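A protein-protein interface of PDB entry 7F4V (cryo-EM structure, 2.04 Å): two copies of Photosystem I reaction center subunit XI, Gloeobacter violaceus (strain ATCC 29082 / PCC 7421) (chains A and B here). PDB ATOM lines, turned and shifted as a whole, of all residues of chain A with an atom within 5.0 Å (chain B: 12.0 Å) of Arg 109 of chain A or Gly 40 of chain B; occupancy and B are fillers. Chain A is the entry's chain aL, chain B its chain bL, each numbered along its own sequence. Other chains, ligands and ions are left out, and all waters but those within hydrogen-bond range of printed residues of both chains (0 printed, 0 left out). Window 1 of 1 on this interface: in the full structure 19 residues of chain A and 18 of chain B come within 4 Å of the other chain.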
ATOM      1  N   ALA A  97       8.854  15.064 -13.651  1.00  0.00           N
ATOM      2  CA  ALA A  97       7.670  14.965 -12.807  1.00  0.00           C
ATOM      3  C   ALA A  97       6.546  14.205 -13.489  1.00  0.00           C
ATOM      4  O   ALA A  97       5.765  13.514 -12.831  1.00  0.00           O
ATOM      5  CB  ALA A  97       7.202  16.364 -12.453  1.00  0.00           C
ATOM      6  N   SER A  98       6.422  14.350 -14.802  1.00  0.00           N
ATOM      7  CA  SER A  98       5.380  13.638 -15.519  1.00  0.00           C
ATOM      8  C   SER A  98       5.676  12.150 -15.639  1.00  0.00           C
ATOM      9  O   SER A  98       4.749  11.363 -15.823  1.00  0.00           O
ATOM     10  CB  SER A  98       5.186  14.256 -16.900  1.00  0.00           C
ATOM     11  OG  SER A  98       4.435  15.449 -16.812  1.00  0.00           O
ATOM     12  N   LEU A  99       6.933  11.744 -15.498  1.00  0.00           N
ATOM     13  CA  LEU A  99       7.339  10.384 -15.814  1.00  0.00           C
ATOM     14  C   LEU A  99       7.705   9.518 -14.612  1.00  0.00           C
ATOM     15  O   LEU A  99       7.963   8.333 -14.815  1.00  0.00           O
ATOM     16  CB  LEU A  99       8.519  10.420 -16.793  1.00  0.00           C
ATOM     17  CG  LEU A  99       8.259  11.120 -18.134  1.00  0.00           C
ATOM     18  CD1 LEU A  99       9.563  11.464 -18.814  1.00  0.00           C
ATOM     19  CD2 LEU A  99       7.369  10.303 -19.057  1.00  0.00           C
ATOM     20  N   VAL A 100       7.699  10.046 -13.379  1.00  0.00           N
ATOM     21  CA  VAL A 100       8.289   9.327 -12.237  1.00  0.00           C
ATOM     22  C   VAL A 100       7.482   8.090 -11.874  1.00  0.00           C
ATOM     23  O   VAL A 100       8.019   6.978 -11.852  1.00  0.00           O
ATOM     24  CB  VAL A 100       8.417  10.223 -10.991  1.00  0.00           C
ATOM     25  CG1 VAL A 100       9.846  10.298 -10.555  1.00  0.00           C
ATOM     26  CG2 VAL A 100       7.779  11.571 -11.152  1.00  0.00           C
ATOM     27  N   GLU A 101       6.222   8.288 -11.476  1.00  0.00           N
ATOM     28  CA  GLU A 101       5.244   7.285 -11.031  1.00  0.00           C
ATOM     29  C   GLU A 101       5.611   6.609  -9.692  1.00  0.00           C
ATOM     30  O   GLU A 101       4.815   5.804  -9.193  1.00  0.00           O
ATOM     31  CB  GLU A 101       4.988   6.215 -12.124  1.00  0.00           C
ATOM     32  CG  GLU A 101       3.698   5.375 -12.085  1.00  0.00           C
ATOM     33  CD  GLU A 101       2.490   6.067 -12.685  1.00  0.00           C
ATOM     34  OE1 GLU A 101       2.172   5.782 -13.861  1.00  0.00           O
ATOM     35  OE2 GLU A 101       1.864   6.888 -11.982  1.00  0.00           O
ATOM     36  N   PHE A 107       7.357  12.499  -3.569  1.00  0.00           N
ATOM     37  CA  PHE A 107       7.745  11.889  -4.831  1.00  0.00           C
ATOM     38  C   PHE A 107       6.542  11.355  -5.584  1.00  0.00           C
ATOM     39  O   PHE A 107       6.687  10.476  -6.438  1.00  0.00           O
ATOM     40  CB  PHE A 107       8.782  10.792  -4.604  1.00  0.00           C
ATOM     41  CG  PHE A 107       9.670  11.060  -3.445  1.00  0.00           C
ATOM     42  CD1 PHE A 107      10.624  12.069  -3.506  1.00  0.00           C
ATOM     43  CD2 PHE A 107       9.523  10.340  -2.268  1.00  0.00           C
ATOM     44  CE1 PHE A 107      11.430  12.335  -2.430  1.00  0.00           C
ATOM     45  CE2 PHE A 107      10.331  10.600  -1.190  1.00  0.00           C
ATOM     46  CZ  PHE A 107      11.292  11.598  -1.272  1.00  0.00           C
ATOM     47  N   ASP A 108       5.357  11.873  -5.274  1.00  0.00           N
ATOM     48  CA  ASP A 108       4.200  11.723  -6.136  1.00  0.00           C
ATOM     49  C   ASP A 108       4.455  12.411  -7.477  1.00  0.00           C
ATOM     50  O   ASP A 108       5.304  13.299  -7.594  1.00  0.00           O
ATOM     51  CB  ASP A 108       2.969  12.326  -5.466  1.00  0.00           C
ATOM     52  CG  ASP A 108       1.692  11.753  -5.991  1.00  0.00           C
ATOM     53  OD1 ASP A 108       1.200  10.776  -5.402  1.00  0.00           O
ATOM     54  OD2 ASP A 108       1.185  12.270  -7.001  1.00  0.00           O
ATOM     55  N   ARG A 109       3.714  11.979  -8.506  1.00  0.00           N
ATOM     56  CA  ARG A 109       3.815  12.639  -9.805  1.00  0.00           C
ATOM     57  C   ARG A 109       3.312  14.069  -9.716  1.00  0.00           C
ATOM     58  O   ARG A 109       3.969  14.995 -10.204  1.00  0.00           O
ATOM     59  CB  ARG A 109       3.046  11.867 -10.882  1.00  0.00           C
ATOM     60  CG  ARG A 109       3.881  10.830 -11.603  1.00  0.00           C
ATOM     61  CD  ARG A 109       3.240  10.338 -12.889  1.00  0.00           C
ATOM     62  NE  ARG A 109       4.124   9.408 -13.587  1.00  0.00           N
ATOM     63  CZ  ARG A 109       3.757   8.616 -14.591  1.00  0.00           C
ATOM     64  NH1 ARG A 109       2.508   8.626 -15.034  1.00  0.00           N
ATOM     65  NH2 ARG A 109       4.640   7.805 -15.147  1.00  0.00           N
ATOM     66  N   LYS A 110       2.161  14.267  -9.060  1.00  0.00           N
ATOM     67  CA  LYS A 110       1.658  15.615  -8.831  1.00  0.00           C
ATOM     68  C   LYS A 110       2.558  16.380  -7.875  1.00  0.00           C
ATOM     69  O   LYS A 110       2.713  17.597  -8.007  1.00  0.00           O
ATOM     70  CB  LYS A 110       0.233  15.577  -8.280  1.00  0.00           C
ATOM     71  CG  LYS A 110      -0.813  15.032  -9.219  1.00  0.00           C
ATOM     72  CD  LYS A 110      -2.158  15.680  -8.914  1.00  0.00           C
ATOM     73  CE  LYS A 110      -3.300  14.943  -9.575  1.00  0.00           C
ATOM     74  NZ  LYS A 110      -4.544  15.779  -9.609  1.00  0.00           N
ATOM     75  N   GLY A 111       3.150  15.680  -6.909  1.00  0.00           N
ATOM     76  CA  GLY A 111       4.082  16.257  -5.966  1.00  0.00           C
ATOM     77  C   GLY A 111       5.300  16.862  -6.624  1.00  0.00           C
ATOM     78  O   GLY A 111       5.589  18.037  -6.409  1.00  0.00           O
ATOM     79  N   TRP A 112       6.002  16.082  -7.448  1.00  0.00           N
ATOM     80  CA  TRP A 112       7.122  16.617  -8.213  1.00  0.00           C
ATOM     81  C   TRP A 112       6.672  17.707  -9.180  1.00  0.00           C
ATOM     82  O   TRP A 112       7.408  18.667  -9.426  1.00  0.00           O
ATOM     83  CB  TRP A 112       7.812  15.498  -8.984  1.00  0.00           C
ATOM     84  CG  TRP A 112       8.835  14.725  -8.247  1.00  0.00           C
ATOM     85  CD1 TRP A 112       8.768  13.421  -7.899  1.00  0.00           C
ATOM     86  CD2 TRP A 112      10.107  15.197  -7.795  1.00  0.00           C
ATOM     87  NE1 TRP A 112       9.908  13.046  -7.243  1.00  0.00           N
ATOM     88  CE2 TRP A 112      10.751  14.118  -7.167  1.00  0.00           C
ATOM     89  CE3 TRP A 112      10.754  16.429  -7.845  1.00  0.00           C
ATOM     90  CZ2 TRP A 112      12.015  14.233  -6.589  1.00  0.00           C
ATOM     91  CZ3 TRP A 112      12.008  16.542  -7.282  1.00  0.00           C
ATOM     92  CH2 TRP A 112      12.623  15.452  -6.656  1.00  0.00           C
ATOM     93  N   SER A 113       5.455  17.586  -9.711  1.00  0.00           N
ATOM     94  CA  SER A 113       4.945  18.567 -10.662  1.00  0.00           C
ATOM     95  C   SER A 113       4.709  19.918  -9.999  1.00  0.00           C
ATOM     96  O   SER A 113       5.034  20.958 -10.571  1.00  0.00           O
ATOM     97  CB  SER A 113       3.671  18.042 -11.310  1.00  0.00           C
ATOM     98  OG  SER A 113       3.157  18.964 -12.239  1.00  0.00           O
ATOM     99  N   ILE B  31      -2.449  16.577 -28.616  1.00  0.00           N
ATOM    100  CA  ILE B  31      -3.505  17.049 -27.721  1.00  0.00           C
ATOM    101  C   ILE B  31      -3.387  16.387 -26.358  1.00  0.00           C
ATOM    102  O   ILE B  31      -3.532  17.045 -25.321  1.00  0.00           O
ATOM    103  CB  ILE B  31      -4.885  16.801 -28.358  1.00  0.00           C
ATOM    104  CG1 ILE B  31      -5.065  17.690 -29.580  1.00  0.00           C
ATOM    105  CG2 ILE B  31      -6.012  17.041 -27.365  1.00  0.00           C
ATOM    106  CD1 ILE B  31      -6.392  17.500 -30.240  1.00  0.00           C
ATOM    107  N   ASP B  32      -3.077  15.083 -26.340  1.00  0.00           N
ATOM    108  CA  ASP B  32      -2.911  14.344 -25.092  1.00  0.00           C
ATOM    109  C   ASP B  32      -1.724  14.826 -24.269  1.00  0.00           C
ATOM    110  O   ASP B  32      -1.669  14.547 -23.070  1.00  0.00           O
ATOM    111  CB  ASP B  32      -2.721  12.848 -25.363  1.00  0.00           C
ATOM    112  CG  ASP B  32      -3.978  12.173 -25.847  1.00  0.00           C
ATOM    113  OD1 ASP B  32      -5.028  12.843 -25.945  1.00  0.00           O
ATOM    114  OD2 ASP B  32      -3.913  10.966 -26.160  1.00  0.00           O
ATOM    115  N   ASN B  33      -0.774  15.523 -24.880  1.00  0.00           N
ATOM    116  CA  ASN B  33       0.408  15.983 -24.176  1.00  0.00           C
ATOM    117  C   ASN B  33       0.483  17.494 -24.048  1.00  0.00           C
ATOM    118  O   ASN B  33       1.478  18.006 -23.532  1.00  0.00           O
ATOM    119  CB  ASN B  33       1.656  15.425 -24.850  1.00  0.00           C
ATOM    120  CG  ASN B  33       1.781  13.935 -24.644  1.00  0.00           C
ATOM    121  OD1 ASN B  33       2.267  13.488 -23.618  1.00  0.00           O
ATOM    122  ND2 ASN B  33       1.299  13.161 -25.601  1.00  0.00           N
ATOM    123  N   LEU B  34      -0.543  18.215 -24.496  1.00  0.00           N
ATOM    124  CA  LEU B  34      -0.764  19.582 -24.053  1.00  0.00           C
ATOM    125  C   LEU B  34      -0.955  19.589 -22.537  1.00  0.00           C
ATOM    126  O   LEU B  34      -1.456  18.610 -21.980  1.00  0.00           O
ATOM    127  CB  LEU B  34      -1.995  20.161 -24.744  1.00  0.00           C
ATOM    128  CG  LEU B  34      -1.913  20.337 -26.260  1.00  0.00           C
ATOM    129  CD1 LEU B  34      -3.191  20.939 -26.800  1.00  0.00           C
ATOM    130  CD2 LEU B  34      -0.709  21.172 -26.648  1.00  0.00           C
ATOM    131  N   PRO B  35      -0.557  20.668 -21.846  1.00  0.00           N
ATOM    132  CA  PRO B  35      -0.536  20.632 -20.371  1.00  0.00           C
ATOM    133  C   PRO B  35      -1.886  20.454 -19.726  1.00  0.00           C
ATOM    134  O   PRO B  35      -1.936  19.987 -18.593  1.00  0.00           O
ATOM    135  CB  PRO B  35       0.081  21.985 -19.987  1.00  0.00           C
ATOM    136  CG  PRO B  35      -0.122  22.830 -21.144  1.00  0.00           C
ATOM    137  CD  PRO B  35      -0.022  21.940 -22.343  1.00  0.00           C
ATOM    138  N   ILE B  36      -2.982  20.760 -20.416  1.00  0.00           N
ATOM    139  CA  ILE B  36      -4.290  20.479 -19.844  1.00  0.00           C
ATOM    140  C   ILE B  36      -4.589  18.979 -19.808  1.00  0.00           C
ATOM    141  O   ILE B  36      -5.362  18.535 -18.959  1.00  0.00           O
ATOM    142  CB  ILE B  36      -5.366  21.281 -20.604  1.00  0.00           C
ATOM    143  CG1 ILE B  36      -6.666  21.369 -19.803  1.00  0.00           C
ATOM    144  CG2 ILE B  36      -5.614  20.732 -21.988  1.00  0.00           C
ATOM    145  CD1 ILE B  36      -6.526  22.064 -18.536  1.00  0.00           C
ATOM    146  N   ASN B  37      -3.952  18.177 -20.663  1.00  0.00           N
ATOM    147  CA  ASN B  37      -4.213  16.746 -20.747  1.00  0.00           C
ATOM    148  C   ASN B  37      -3.035  15.868 -20.348  1.00  0.00           C
ATOM    149  O   ASN B  37      -3.220  14.656 -20.215  1.00  0.00           O
ATOM    150  CB  ASN B  37      -4.626  16.362 -22.175  1.00  0.00           C
ATOM    151  CG  ASN B  37      -5.877  17.070 -22.632  1.00  0.00           C
ATOM    152  OD1 ASN B  37      -6.832  17.197 -21.881  1.00  0.00           O
ATOM    153  ND2 ASN B  37      -5.874  17.532 -23.871  1.00  0.00           N
ATOM    154  N   ARG B  38      -1.843  16.435 -20.178  1.00  0.00           N
ATOM    155  CA  ARG B  38      -0.626  15.646 -20.028  1.00  0.00           C
ATOM    156  C   ARG B  38      -0.622  14.861 -18.720  1.00  0.00           C
ATOM    157  O   ARG B  38      -0.921  15.402 -17.654  1.00  0.00           O
ATOM    158  CB  ARG B  38       0.597  16.557 -20.095  1.00  0.00           C
ATOM    159  CG  ARG B  38       1.942  15.858 -20.002  1.00  0.00           C
ATOM    160  CD  ARG B  38       3.053  16.878 -19.935  1.00  0.00           C
ATOM    161  NE  ARG B  38       2.825  17.930 -20.907  1.00  0.00           N
ATOM    162  CZ  ARG B  38       3.195  19.192 -20.757  1.00  0.00           C
ATOM    163  NH1 ARG B  38       3.833  19.589 -19.666  1.00  0.00           N
ATOM    164  NH2 ARG B  38       2.901  20.062 -21.701  1.00  0.00           N
ATOM    165  N   VAL B  39      -0.277  13.578 -18.825  1.00  0.00           N
ATOM    166  CA  VAL B  39      -0.265  12.676 -17.684  1.00  0.00           C
ATOM    167  C   VAL B  39       0.806  13.095 -16.679  1.00  0.00           C
ATOM    168  O   VAL B  39       1.916  13.491 -17.051  1.00  0.00           O
ATOM    169  CB  VAL B  39      -0.059  11.242 -18.209  1.00  0.00           C
ATOM    170  CG1 VAL B  39       0.533  10.315 -17.173  1.00  0.00           C
ATOM    171  CG2 VAL B  39      -1.372  10.682 -18.723  1.00  0.00           C
ATOM    172  N   GLY B  40       0.453  13.051 -15.397  1.00  0.00           N
ATOM    173  CA  GLY B  40       1.408  13.216 -14.327  1.00  0.00           C
ATOM    174  C   GLY B  40       1.567  14.626 -13.818  1.00  0.00           C
ATOM    175  O   GLY B  40       2.370  14.850 -12.907  1.00  0.00           O
ATOM    176  N   MET B  41       0.830  15.578 -14.365  1.00  0.00           N
ATOM    177  CA  MET B  41       0.967  16.965 -13.966  1.00  0.00           C
ATOM    178  C   MET B  41       0.023  17.292 -12.821  1.00  0.00           C
ATOM    179  O   MET B  41      -1.067  16.729 -12.704  1.00  0.00           O
ATOM    180  CB  MET B  41       0.677  17.903 -15.136  1.00  0.00           C
ATOM    181  CG  MET B  41       1.648  17.805 -16.287  1.00  0.00           C
ATOM    182  SD  MET B  41       1.295  19.054 -17.532  1.00  0.00           S
ATOM    183  CE  MET B  41       2.082  20.497 -16.838  1.00  0.00           C
ATOM    184  N   ASP B  42       0.444  18.232 -11.993  1.00  0.00           N
ATOM    185  CA  ASP B  42      -0.471  18.868 -11.071  1.00  0.00           C
ATOM    186  C   ASP B  42      -1.147  20.030 -11.770  1.00  0.00           C
ATOM    187  O   ASP B  42      -0.561  20.679 -12.636  1.00  0.00           O
ATOM    188  CB  ASP B  42       0.221  19.373  -9.814  1.00  0.00           C
ATOM    189  CG  ASP B  42      -0.777  19.842  -8.773  1.00  0.00           C
ATOM    190  OD1 ASP B  42      -1.246  19.010  -7.976  1.00  0.00           O
ATOM    191  OD2 ASP B  42      -1.112  21.041  -8.774  1.00  0.00           O
ATOM    192  N   GLU B  43      -2.393  20.281 -11.364  1.00  0.00           N
ATOM    193  CA  GLU B  43      -3.228  21.307 -11.968  1.00  0.00           C
ATOM    194  C   GLU B  43      -2.619  22.701 -11.874  1.00  0.00           C
ATOM    195  O   GLU B  43      -2.870  23.527 -12.752  1.00  0.00           O
ATOM    196  CB  GLU B  43      -4.607  21.278 -11.314  1.00  0.00           C
ATOM    197  CG  GLU B  43      -5.363  19.971 -11.469  1.00  0.00           C
ATOM    198  CD  GLU B  43      -5.085  18.967 -10.348  1.00  0.00           C
ATOM    199  OE1 GLU B  43      -4.169  19.194  -9.530  1.00  0.00           O
ATOM    200  OE2 GLU B  43      -5.792  17.946 -10.287  1.00  0.00           O
ATOM    201  N   PHE B  44      -1.803  22.976 -10.847  1.00  0.00           N
ATOM    202  CA  PHE B  44      -1.070  24.240 -10.812  1.00  0.00           C
ATOM    203  C   PHE B  44      -0.090  24.337 -11.975  1.00  0.00           C
ATOM    204  O   PHE B  44      -0.037  25.356 -12.666  1.00  0.00           O
ATOM    205  CB  PHE B  44      -0.304  24.425  -9.496  1.00  0.00           C
ATOM    206  CG  PHE B  44       0.598  25.636  -9.517  1.00  0.00           C
ATOM    207  CD1 PHE B  44       0.063  26.893  -9.343  1.00  0.00           C
ATOM    208  CD2 PHE B  44       1.969  25.529  -9.766  1.00  0.00           C
ATOM    209  CE1 PHE B  44       0.866  28.014  -9.399  1.00  0.00           C
ATOM    210  CE2 PHE B  44       2.761  26.648  -9.840  1.00  0.00           C
ATOM    211  CZ  PHE B  44       2.196  27.898  -9.655  1.00  0.00           C
ATOM    212  N   THR B  45       0.733  23.300 -12.157  1.00  0.00           N
ATOM    213  CA  THR B  45       1.729  23.303 -13.222  1.00  0.00           C
ATOM    214  C   THR B  45       1.065  23.252 -14.592  1.00  0.00           C
ATOM    215  O   THR B  45       1.604  23.805 -15.555  1.00  0.00           O
ATOM    216  CB  THR B  45       2.703  22.137 -13.019  1.00  0.00           C
ATOM    217  OG1 THR B  45       3.159  22.132 -11.659  1.00  0.00           O
ATOM    218  CG2 THR B  45       3.916  22.238 -13.935  1.00  0.00           C
ATOM    219  N   ARG B  46      -0.116  22.627 -14.681  1.00  0.00           N
ATOM    220  CA  ARG B  46      -0.942  22.726 -15.881  1.00  0.00           C
ATOM    221  C   ARG B  46      -1.285  24.175 -16.180  1.00  0.00           C
ATOM    222  O   ARG B  46      -1.030  24.664 -17.281  1.00  0.00           O
ATOM    223  CB  ARG B  46      -2.234  21.923 -15.725  1.00  0.00           C
ATOM    224  CG  ARG B  46      -2.070  20.459 -15.467  1.00  0.00           C
ATOM    225  CD  ARG B  46      -3.378  19.723 -15.650  1.00  0.00           C
ATOM    226  NE  ARG B  46      -3.254  18.331 -15.250  1.00  0.00           N
ATOM    227  CZ  ARG B  46      -2.836  17.365 -16.051  1.00  0.00           C
ATOM    228  NH1 ARG B  46      -2.509  17.642 -17.303  1.00  0.00           N
ATOM    229  NH2 ARG B  46      -2.740  16.127 -15.599  1.00  0.00           N
ATOM    230  N   GLY B  47      -1.841  24.875 -15.189  1.00  0.00           N
ATOM    231  CA  GLY B  47      -2.220  26.263 -15.383  1.00  0.00           C
ATOM    232  C   GLY B  47      -1.027  27.155 -15.643  1.00  0.00           C
ATOM    233  O   GLY B  47      -1.098  28.059 -16.474  1.00  0.00           O
ATOM    234  N   GLU B  49       1.844  26.408 -17.193  1.00  0.00           N
ATOM    235  CA  GLU B  49       2.304  26.287 -18.572  1.00  0.00           C
ATOM    236  C   GLU B  49       1.318  26.922 -19.545  1.00  0.00           C
ATOM    237  O   GLU B  49       1.726  27.552 -20.521  1.00  0.00           O
ATOM    238  CB  GLU B  49       2.530  24.818 -18.933  1.00  0.00           C
ATOM    239  CG  GLU B  49       3.187  24.629 -20.295  1.00  0.00           C
ATOM    240  CD  GLU B  49       3.409  23.177 -20.661  1.00  0.00           C
ATOM    241  OE1 GLU B  49       3.457  22.332 -19.759  1.00  0.00           O
ATOM    242  OE2 GLU B  49       3.548  22.888 -21.860  1.00  0.00           O
ATOM    243  N   THR B 105     -10.134  14.156 -10.299  1.00  0.00           N
ATOM    244  CA  THR B 105      -8.904  14.917 -10.068  1.00  0.00           C
ATOM    245  C   THR B 105      -8.697  16.264 -10.762  1.00  0.00           C
ATOM    246  O   THR B 105      -8.578  17.274 -10.066  1.00  0.00           O
ATOM    247  CB  THR B 105      -7.722  14.024 -10.457  1.00  0.00           C
ATOM    248  OG1 THR B 105      -7.810  13.708 -11.855  1.00  0.00           O
ATOM    249  CG2 THR B 105      -7.739  12.730  -9.642  1.00  0.00           C
ATOM    250  N   GLU B 106      -8.649  16.330 -12.097  1.00  0.00           N
ATOM    251  CA  GLU B 106      -8.369  17.631 -12.707  1.00  0.00           C
ATOM    252  C   GLU B 106      -9.599  18.521 -12.718  1.00  0.00           C
ATOM    253  O   GLU B 106      -9.469  19.747 -12.684  1.00  0.00           O
ATOM    254  CB  GLU B 106      -7.834  17.470 -14.132  1.00  0.00           C
ATOM    255  CG  GLU B 106      -6.955  18.609 -14.617  1.00  0.00           C
ATOM    256  CD  GLU B 106      -7.711  19.659 -15.413  1.00  0.00           C
ATOM    257  OE1 GLU B 106      -8.078  19.382 -16.569  1.00  0.00           O
ATOM    258  OE2 GLU B 106      -7.959  20.755 -14.885  1.00  0.00           O
ATOM    259  N   ARG B 114      -6.584  25.437  -8.469  1.00  0.00           N
ATOM    260  CA  ARG B 114      -5.136  25.490  -8.638  1.00  0.00           C
ATOM    261  C   ARG B 114      -4.747  25.822 -10.068  1.00  0.00           C
ATOM    262  O   ARG B 114      -3.726  26.474 -10.289  1.00  0.00           O
ATOM    263  CB  ARG B 114      -4.498  24.166  -8.224  1.00  0.00           C
ATOM    264  CG  ARG B 114      -3.969  24.213  -6.836  1.00  0.00           C
ATOM    265  CD  ARG B 114      -3.055  23.061  -6.409  1.00  0.00           C
ATOM    266  NE  ARG B 114      -3.347  21.768  -7.015  1.00  0.00           N
ATOM    267  CZ  ARG B 114      -4.291  20.928  -6.604  1.00  0.00           C
ATOM    268  NH1 ARG B 114      -4.446  19.771  -7.223  1.00  0.00           N
ATOM    269  NH2 ARG B 114      -5.070  21.226  -5.577  1.00  0.00           N
ATOM    270  N   LEU B 115      -5.544  25.374 -11.039  1.00  0.00           N
ATOM    271  CA  LEU B 115      -5.292  25.737 -12.424  1.00  0.00           C
ATOM    272  C   LEU B 115      -5.486  27.229 -12.642  1.00  0.00           C
ATOM    273  O   LEU B 115      -4.693  27.856 -13.346  1.00  0.00           O
ATOM    274  CB  LEU B 115      -6.195  24.934 -13.357  1.00  0.00           C
ATOM    275  CG  LEU B 115      -5.736  25.075 -14.803  1.00  0.00           C
ATOM    276  CD1 LEU B 115      -5.492  23.713 -15.381  1.00  0.00           C
ATOM    277  CD2 LEU B 115      -6.734  25.864 -15.625  1.00  0.00           C
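No position is printed for both chains.
Among the printed residues, merely in contact across the chains: Arg 109 of chain A with Val 39 of chain B (3.4 Å), Ser 113 of chain A with Met 41 of chain B (3.4 Å), Lys 110 of chain A with Asp 42 of chain B (3.6 Å), Ala 97 of chain A with Gly 40 of chain B (3.6 Å), Ser 98 of chain A with Met 41 of chain B (3.7 Å), Ser 98 of chain A with Arg 38 of chain B (3.7 Å), Lys 110 of chain A with Thr 105 of chain B (3.7 Å), Ser 113 of chain A with Gly 40 of chain B (3.8 Å), Lys 110 of chain A with Met 41 of chain B (3.9 Å) and Lys 110 of chain A with Gly 40 of chain B (3.9 Å).
Along chain B the printed residues that touch a printed residue of chain A span positions 38 to 105.
Of the 12 printed residues of chain A, 5 touch a printed residue of chain B.
Along chain A the printed residues that touch a printed residue of chain B span positions 97 to 113.
Among the printed residues, 15 pairs touch across the chains.
Among the printed residues, Asp or Glu carboxylates within 4 Å of a Lys or Arg side-chain nitrogen of the other chain: Lys 110 of chain A with Glu 43 of chain B.
Of chain B, only Gly 40 (3.6 Å) comes within 4 Å of Ala 97 of chain A.
No residue of chain B comes within 4 Å of Leu 99 of chain A.
No residue of chain B comes within 4 Å of Glu 101 of chain A.
No residue of chain B comes within 4 Å of Asp 108 of chain A.
Of chain B, only Val 39 and Gly 40 come within 4 Å of Arg 109 of chain A.
Of chain B, only Gly 40 (3.9 Å), Met 41 (3.9 Å), Asp 42 (3.6 Å), Glu 43 (2.6 Å) and Thr 105 (3.7 Å) come within 4 Å of Lys 110 of chain A.
Gly 111 of chain A touches none of the printed residues of chain B.
Ser 113 of chain A touches just these residues of chain B: Gly 40 (3.8 Å), Met 41 (3.4 Å), Asp 42 (2.8 Å) and Thr 45 (2.5 Å).
Gly 40 of chain B touches four residues of chain A.
Printed residues of chain A within 4 Å of Asp 42 of chain B: Lys 110 (3.6 Å) and Ser 113 (2.8 Å).
Printed residues of chain A within 4 Å of Thr 45 of chain B: Ser 113.
Printed residues of chain A within 4 Å of Thr 105 of chain B: Lys 110.
The nearest residue of chain A that does not touch Gly 40 of chain B is Ser 98 of chain A (4.1 Å).
The backbone carbonyl oxygen (O) of Val 39 of chain B lies within hydrogen-bond range of the side-chain hydroxyl (OG) of Ser 98 of chain A (3.2 Å).
NZ of Lys 110 of chain A lies within salt-bridge range of OE2 of Glu 43 of chain B (2.6 Å).
The side-chain hydroxyl (OG) of Ser 113 of chain A sits at hydrogen-bond distance from the backbone NH (N) of Asp 42 of chain B, at 2.8 Å.
O of Ser 113 of chain A sits at hydrogen-bond distance from OG1 of Thr 45 of chain B.
O of Arg 109 of chain A sits close to O of Gly 40 of chain B (3.1 Å).
O of Leu 99 of chain A lies within hydrogen-bond range of NH2 of Arg 109 of chain A, at 3.4 Å.
O of Asp 32 of chain B lies close to N of Arg 38 of chain B (3.5 Å).
The guanidinium group of Arg 38 of chain B lies within hydrogen-bond range of the side-chain sulfur of Met 41 of chain B (3.4 Å).
NH2 of Arg 46 of chain B lies within hydrogen-bond range of O of Met 41 of chain B (3.4 Å).
N of Phe 44 of chain B is in hydrogen-bond range of OD2 of Asp 42 of chain B (2.9 Å).
The side-chain carboxylate (OE1) of Glu 43 of chain B is in salt-bridge range of the guanidinium group (NE) of Arg 114 of chain B (3.7 Å).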
